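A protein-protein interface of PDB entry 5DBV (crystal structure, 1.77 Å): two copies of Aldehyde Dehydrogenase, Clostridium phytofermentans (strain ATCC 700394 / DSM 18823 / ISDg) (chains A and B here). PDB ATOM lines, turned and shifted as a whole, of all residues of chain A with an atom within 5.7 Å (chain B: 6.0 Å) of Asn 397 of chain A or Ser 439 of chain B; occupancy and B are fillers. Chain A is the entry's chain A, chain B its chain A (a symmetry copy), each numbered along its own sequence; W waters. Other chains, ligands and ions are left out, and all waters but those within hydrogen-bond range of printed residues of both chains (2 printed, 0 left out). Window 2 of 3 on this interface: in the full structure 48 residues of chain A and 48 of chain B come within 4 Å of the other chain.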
ATOM      1  N   ALA A 231      -8.576  12.513  18.381  1.00  0.00           N
ATOM      2  CA  ALA A 231      -9.082  13.272  19.524  1.00  0.00           C
ATOM      3  C   ALA A 231     -10.556  13.046  19.800  1.00  0.00           C
ATOM      4  O   ALA A 231     -11.327  12.667  18.918  1.00  0.00           O
ATOM      5  CB  ALA A 231      -8.850  14.733  19.318  1.00  0.00           C
ATOM      6  N   LYS A 235     -15.281  17.101  23.061  1.00  0.00           N
ATOM      7  CA  LYS A 235     -14.573  17.672  24.196  1.00  0.00           C
ATOM      8  C   LYS A 235     -13.480  18.643  23.756  1.00  0.00           C
ATOM      9  O   LYS A 235     -13.225  19.633  24.438  1.00  0.00           O
ATOM     10  CB  LYS A 235     -13.956  16.574  25.069  1.00  0.00           C
ATOM     11  CG  LYS A 235     -13.247  17.125  26.291  1.00  0.00           C
ATOM     12  CD  LYS A 235     -12.892  16.036  27.290  1.00  0.00           C
ATOM     13  CE  LYS A 235     -12.085  16.592  28.472  1.00  0.00           C
ATOM     14  NZ  LYS A 235     -10.716  17.102  28.098  1.00  0.00           N
ATOM     15  N   ASP A 239     -13.077  22.330  25.334  1.00  0.00           N
ATOM     16  CA  ASP A 239     -11.827  22.718  25.989  1.00  0.00           C
ATOM     17  C   ASP A 239     -11.181  23.921  25.308  1.00  0.00           C
ATOM     18  O   ASP A 239     -10.697  24.849  25.968  1.00  0.00           O
ATOM     19  CB  ASP A 239     -10.812  21.568  25.988  1.00  0.00           C
ATOM     20  CG  ASP A 239     -11.115  20.478  26.976  1.00  0.00           C
ATOM     21  OD1 ASP A 239     -11.975  20.626  27.877  1.00  0.00           O
ATOM     22  OD2 ASP A 239     -10.449  19.413  26.826  1.00  0.00           O
ATOM     23  N   ILE A 374      -2.398  20.378  22.453  1.00  0.00           N
ATOM     24  CA  ILE A 374      -2.813  19.338  21.504  1.00  0.00           C
ATOM     25  C   ILE A 374      -3.942  18.517  22.061  1.00  0.00           C
ATOM     26  O   ILE A 374      -4.005  18.263  23.273  1.00  0.00           O
ATOM     27  CB  ILE A 374      -1.618  18.406  21.125  1.00  0.00           C
ATOM     28  CG1 ILE A 374      -2.045  17.352  20.114  1.00  0.00           C
ATOM     29  CG2 ILE A 374      -1.051  17.766  22.360  1.00  0.00           C
ATOM     30  CD1 ILE A 374      -0.869  16.606  19.443  1.00  0.00           C
ATOM     31  N   HIS A 375      -4.850  18.141  21.165  1.00  0.00           N
ATOM     32  CA  HIS A 375      -5.886  17.156  21.458  1.00  0.00           C
ATOM     33  C   HIS A 375      -5.617  15.963  20.556  1.00  0.00           C
ATOM     34  O   HIS A 375      -5.683  16.061  19.334  1.00  0.00           O
ATOM     35  CB  HIS A 375      -7.295  17.738  21.253  1.00  0.00           C
ATOM     36  CG  HIS A 375      -7.629  18.789  22.256  1.00  0.00           C
ATOM     37  ND1 HIS A 375      -8.401  18.538  23.370  1.00  0.00           N
ATOM     38  CD2 HIS A 375      -7.233  20.084  22.348  1.00  0.00           C
ATOM     39  CE1 HIS A 375      -8.463  19.636  24.104  1.00  0.00           C
ATOM     40  NE2 HIS A 375      -7.758  20.584  23.508  1.00  0.00           N
ATOM     41  N   SER A 376      -5.268  14.851  21.198  1.00  0.00           N
ATOM     42  CA  SER A 376      -4.877  13.614  20.534  1.00  0.00           C
ATOM     43  C   SER A 376      -4.837  12.549  21.606  1.00  0.00           C
ATOM     44  O   SER A 376      -4.443  12.837  22.739  1.00  0.00           O
ATOM     45  CB  SER A 376      -3.499  13.720  19.879  1.00  0.00           C
ATOM     46  OG  SER A 376      -3.171  12.501  19.234  1.00  0.00           O
ATOM     47  N   LYS A 377      -5.243  11.338  21.272  1.00  0.00           N
ATOM     48  CA  LYS A 377      -5.128  10.244  22.225  1.00  0.00           C
ATOM     49  C   LYS A 377      -3.932   9.351  21.911  1.00  0.00           C
ATOM     50  O   LYS A 377      -3.743   8.312  22.560  1.00  0.00           O
ATOM     51  CB  LYS A 377      -6.424   9.427  22.237  1.00  0.00           C
ATOM     52  CG  LYS A 377      -7.657  10.201  22.731  1.00  0.00           C
ATOM     53  CD  LYS A 377      -7.445  10.821  24.123  1.00  0.00           C
ATOM     54  CE  LYS A 377      -8.665  11.649  24.599  1.00  0.00           C
ATOM     55  NZ  LYS A 377      -9.838  10.823  24.985  1.00  0.00           N
ATOM     56  N   ILE A 382       1.578  12.659  20.173  1.00  0.00           N
ATOM     57  CA  ILE A 382       1.811  13.620  21.230  1.00  0.00           C
ATOM     58  C   ILE A 382       3.316  13.882  21.371  1.00  0.00           C
ATOM     59  O   ILE A 382       3.758  15.026  21.501  1.00  0.00           O
ATOM     60  CB  ILE A 382       1.230  13.133  22.535  1.00  0.00           C
ATOM     61  CG1 ILE A 382      -0.292  13.243  22.500  1.00  0.00           C
ATOM     62  CG2 ILE A 382       1.748  13.948  23.698  1.00  0.00           C
ATOM     63  CD1 ILE A 382      -0.976  12.494  23.653  1.00  0.00           C
ATOM     64  N   VAL A 395       0.103  21.497  26.804  1.00  0.00           N
ATOM     65  CA  VAL A 395      -1.088  20.896  27.425  1.00  0.00           C
ATOM     66  C   VAL A 395      -1.713  19.918  26.442  1.00  0.00           C
ATOM     67  O   VAL A 395      -1.926  20.241  25.255  1.00  0.00           O
ATOM     68  CB  VAL A 395      -2.126  21.960  27.854  1.00  0.00           C
ATOM     69  CG1 VAL A 395      -3.399  21.320  28.434  1.00  0.00           C
ATOM     70  CG2 VAL A 395      -1.493  22.919  28.856  1.00  0.00           C
ATOM     71  N   LYS A 396      -2.017  18.727  26.955  1.00  0.00           N
ATOM     72  CA  LYS A 396      -2.579  17.637  26.168  1.00  0.00           C
ATOM     73  C   LYS A 396      -3.977  17.295  26.687  1.00  0.00           C
ATOM     74  O   LYS A 396      -4.134  16.924  27.844  1.00  0.00           O
ATOM     75  CB  LYS A 396      -1.684  16.417  26.226  1.00  0.00           C
ATOM     76  CG  LYS A 396      -0.237  16.656  25.683  1.00  0.00           C
ATOM     77  CD  LYS A 396       0.855  15.821  26.397  1.00  0.00           C
ATOM     78  CE  LYS A 396       1.110  16.338  27.805  1.00  0.00           C
ATOM     79  NZ  LYS A 396       2.234  15.664  28.557  1.00  0.00           N
ATOM     80  N   ASN A 397      -4.965  17.453  25.813  1.00  0.00           N
ATOM     81  CA  ASN A 397      -6.359  17.108  26.074  1.00  0.00           C
ATOM     82  C   ASN A 397      -7.003  17.829  27.253  1.00  0.00           C
ATOM     83  O   ASN A 397      -7.773  17.227  28.020  1.00  0.00           O
ATOM     84  CB  ASN A 397      -6.475  15.602  26.263  1.00  0.00           C
ATOM     85  CG  ASN A 397      -5.902  14.834  25.079  1.00  0.00           C
ATOM     86  OD1 ASN A 397      -6.203  15.135  23.929  1.00  0.00           O
ATOM     87  ND2 ASN A 397      -5.039  13.857  25.364  1.00  0.00           N
ATOM     88  N   ALA A 398      -6.732  19.126  27.331  1.00  0.00           N
ATOM     89  CA  ALA A 398      -7.398  20.010  28.289  1.00  0.00           C
ATOM     90  C   ALA A 398      -7.313  21.434  27.803  1.00  0.00           C
ATOM     91  O   ALA A 398      -6.525  21.744  26.900  1.00  0.00           O
ATOM     92  CB  ALA A 398      -6.759  19.884  29.671  1.00  0.00           C
ATOM     93  N   PRO A 399      -8.096  22.329  28.431  1.00  0.00           N
ATOM     94  CA  PRO A 399      -7.866  23.746  28.149  1.00  0.00           C
ATOM     95  C   PRO A 399      -6.479  24.187  28.576  1.00  0.00           C
ATOM     96  O   PRO A 399      -5.865  23.621  29.497  1.00  0.00           O
ATOM     97  CB  PRO A 399      -8.924  24.464  28.992  1.00  0.00           C
ATOM     98  CG  PRO A 399      -9.920  23.407  29.419  1.00  0.00           C
ATOM     99  CD  PRO A 399      -9.123  22.125  29.474  1.00  0.00           C
ATOM    100  N   ALA A 402      -5.081  24.450  32.226  1.00  0.00           N
ATOM    101  CA  ALA A 402      -4.561  23.307  32.985  1.00  0.00           C
ATOM    102  C   ALA A 402      -3.081  23.430  33.243  1.00  0.00           C
ATOM    103  O   ALA A 402      -2.571  22.825  34.189  1.00  0.00           O
ATOM    104  CB  ALA A 402      -4.859  21.980  32.274  1.00  0.00           C
ATOM    105  N   GLY A 407      -7.421  22.465  36.666  1.00  0.00           N
ATOM    106  CA  GLY A 407      -7.742  21.226  35.971  1.00  0.00           C
ATOM    107  C   GLY A 407      -6.539  20.447  35.441  1.00  0.00           C
ATOM    108  O   GLY A 407      -6.676  19.596  34.552  1.00  0.00           O
ATOM    109  N   ARG B 100      -6.355  14.251  37.919  1.00  0.00           N
ATOM    110  CA  ARG B 100      -6.289  15.173  36.769  1.00  0.00           C
ATOM    111  C   ARG B 100      -5.206  14.813  35.772  1.00  0.00           C
ATOM    112  O   ARG B 100      -4.955  15.567  34.811  1.00  0.00           O
ATOM    113  CB  ARG B 100      -6.079  16.609  37.250  1.00  0.00           C
ATOM    114  CG  ARG B 100      -7.310  17.142  38.030  1.00  0.00           C
ATOM    115  CD  ARG B 100      -6.974  18.340  38.903  1.00  0.00           C
ATOM    116  NE  ARG B 100      -5.883  18.069  39.840  1.00  0.00           N
ATOM    117  CZ  ARG B 100      -5.187  19.013  40.463  1.00  0.00           C
ATOM    118  NH1 ARG B 100      -5.466  20.293  40.246  1.00  0.00           N
ATOM    119  NH2 ARG B 100      -4.214  18.682  41.298  1.00  0.00           N
ATOM    120  N   GLY B 101      -4.562  13.664  35.976  1.00  0.00           N
ATOM    121  CA  GLY B 101      -3.598  13.173  35.004  1.00  0.00           C
ATOM    122  C   GLY B 101      -2.158  13.204  35.455  1.00  0.00           C
ATOM    123  O   GLY B 101      -1.845  12.921  36.612  1.00  0.00           O
ATOM    124  N   LEU B 102      -1.271  13.507  34.521  1.00  0.00           N
ATOM    125  CA  LEU B 102       0.168  13.449  34.753  1.00  0.00           C
ATOM    126  C   LEU B 102       0.790  14.722  34.278  1.00  0.00           C
ATOM    127  O   LEU B 102       0.547  15.109  33.139  1.00  0.00           O
ATOM    128  CB  LEU B 102       0.795  12.275  34.003  1.00  0.00           C
ATOM    129  CG  LEU B 102       2.327  12.260  34.029  1.00  0.00           C
ATOM    130  CD1 LEU B 102       2.895  11.942  35.393  1.00  0.00           C
ATOM    131  CD2 LEU B 102       2.810  11.234  32.999  1.00  0.00           C
ATOM    132  N   VAL B 437       1.557  18.776  30.418  1.00  0.00           N
ATOM    133  CA  VAL B 437       0.364  18.453  31.207  1.00  0.00           C
ATOM    134  C   VAL B 437      -0.509  17.496  30.434  1.00  0.00           C
ATOM    135  O   VAL B 437      -1.179  17.895  29.471  1.00  0.00           O
ATOM    136  CB  VAL B 437      -0.463  19.733  31.536  1.00  0.00           C
ATOM    137  CG1 VAL B 437      -1.695  19.411  32.410  1.00  0.00           C
ATOM    138  CG2 VAL B 437       0.430  20.782  32.186  1.00  0.00           C
ATOM    139  N   MET B 438      -0.524  16.246  30.892  1.00  0.00           N
ATOM    140  CA  MET B 438      -1.306  15.179  30.279  1.00  0.00           C
ATOM    141  C   MET B 438      -2.574  15.061  31.095  1.00  0.00           C
ATOM    142  O   MET B 438      -2.574  14.518  32.192  1.00  0.00           O
ATOM    143  CB  MET B 438      -0.521  13.857  30.267  1.00  0.00           C
ATOM    144  CG  MET B 438      -1.298  12.686  29.668  1.00  0.00           C
ATOM    145  SD  MET B 438      -1.348  12.734  27.855  1.00  0.00           S
ATOM    146  CE  MET B 438       0.381  12.417  27.499  1.00  0.00           C
ATOM    147  N   SER B 439      -3.649  15.598  30.567  1.00  0.00           N
ATOM    148  CA  SER B 439      -4.837  15.793  31.360  1.00  0.00           C
ATOM    149  C   SER B 439      -5.701  14.562  31.384  1.00  0.00           C
ATOM    150  O   SER B 439      -6.106  14.037  30.339  1.00  0.00           O
ATOM    151  CB  SER B 439      -5.645  16.973  30.829  1.00  0.00           C
ATOM    152  OG  SER B 439      -6.895  17.017  31.494  1.00  0.00           O
ATOM    153  N   ASP B 440      -5.996  14.128  32.605  1.00  0.00           N
ATOM    154  CA  ASP B 440      -6.972  13.094  32.872  1.00  0.00           C
ATOM    155  C   ASP B 440      -6.541  11.773  32.286  1.00  0.00           C
ATOM    156  O   ASP B 440      -7.380  10.946  31.959  1.00  0.00           O
ATOM    157  CB  ASP B 440      -8.359  13.490  32.336  1.00  0.00           C
ATOM    158  CG  ASP B 440      -8.954  14.687  33.065  1.00  0.00           C
ATOM    159  OD1 ASP B 440      -8.468  15.009  34.159  1.00  0.00           O
ATOM    160  OD2 ASP B 440      -9.915  15.304  32.547  1.00  0.00           O
ATOM    161  N   SER B 441      -5.234  11.568  32.171  1.00  0.00           N
ATOM    162  CA  SER B 441      -4.714  10.236  31.851  1.00  0.00           C
ATOM    163  C   SER B 441      -3.294  10.035  32.379  1.00  0.00           C
ATOM    164  O   SER B 441      -2.597  10.983  32.768  1.00  0.00           O
ATOM    165  CB  SER B 441      -4.743   9.969  30.342  1.00  0.00           C
ATOM    166  OG  SER B 441      -3.733  10.709  29.671  1.00  0.00           O
HETATM  167  O   HOH W   1      -4.934  12.691  28.083  1.00  0.00           O
HETATM  168  O   HOH W   2      -9.493  17.554  30.683  1.00  0.00           O
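Among the printed residues, no Asp or Glu carboxylate lies within 4 Å of a Lys or Arg side-chain nitrogen of the other chain.
Asp 239 of chain A touches none of the printed residues of chain B. Of the printed residues of chain B, Val 395 of chain A touches Val 437 (3.6 Å). Of chain B, only Ser 439 (3.5 Å) comes within 4 Å of Asn 397 of chain A. Of the printed residues of chain B, Ala 398 of chain A touches Ser 439. Of the printed residues of chain B, Ala 402 of chain A touches Val 437. Printed residues of chain A within 4 Å of Met 438 of chain B: Lys 396 (3.5 Å). Of the printed residues of chain A, Ser 439 of chain B touches Lys 396, Asn 397 and Ala 398. The nearest residue of chain B that does not touch Asn 397 of chain A is Met 438 of chain B (4.6 Å).
The side-chain amino group of Lys 235 of chain A sits at hydrogen-bond distance from the backbone carbonyl oxygen of Asn 397 of chain A (2.9 Å). The backbone NH of Ile 374 of chain A lies within hydrogen-bond range of the backbone carbonyl oxygen of Val 395 of chain A. The backbone NH (N) of Asn 397 of chain A sits at hydrogen-bond distance from the backbone carbonyl oxygen (O) of Ile 374 of chain A, at 2.8 Å. O of Ser 376 of chain A lies within hydrogen-bond range of ND2 of Asn 397 of chain A. The backbone carbonyl oxygen of Leu 102 of chain B is in hydrogen-bond range of the backbone NH of Met 438 of chain B, at 2.7 Å. SD of Met 438 of chain B lies close to OG of Ser 441 of chain B.
Water W2 lies within hydrogen-bond range of the side-chain hydroxyl of Ser 439 of chain B, the side-chain amino group of Lys 235 of chain A, the side-chain carboxylate of Asp 440 of chain B and the backbone carbonyl oxygen of Asn 397 of chain A. Water W1 lies within hydrogen-bond range of OG of Ser 441 of chain B (2.8 Å), O of Ser 439 of chain B (2.9 Å), ND2 of Asn 397 of chain A (3.0 Å) and SD of Met 438 of chain B (3.6 Å).
No position is printed for both chains. Of the 7 pairs that touch across the chains among the printed residues, none has its exchanged pair printed and touching as well.
The backbone carbonyl oxygen (O) of Val 437 of chain B sits at hydrogen-bond distance from the backbone NH (N) of Lys 396 of chain A (2.8 Å). O of Lys 396 of chain A lies within hydrogen-bond range of N of Ser 439 of chain B, at 3.1 Å.
Among the printed residues, merely in contact across the chains: Val 395 of chain A with Val 437 of chain B (3.6 Å), Lys 396 of chain A with Met 438 of chain B (3.5 Å), Asn 397 of chain A with Ser 439 of chain B (3.5 Å), Ala 398 of chain A with Ser 439 of chain B (3.3 Å) and Ala 402 of chain A with Val 437 of chain B (3.9 Å).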
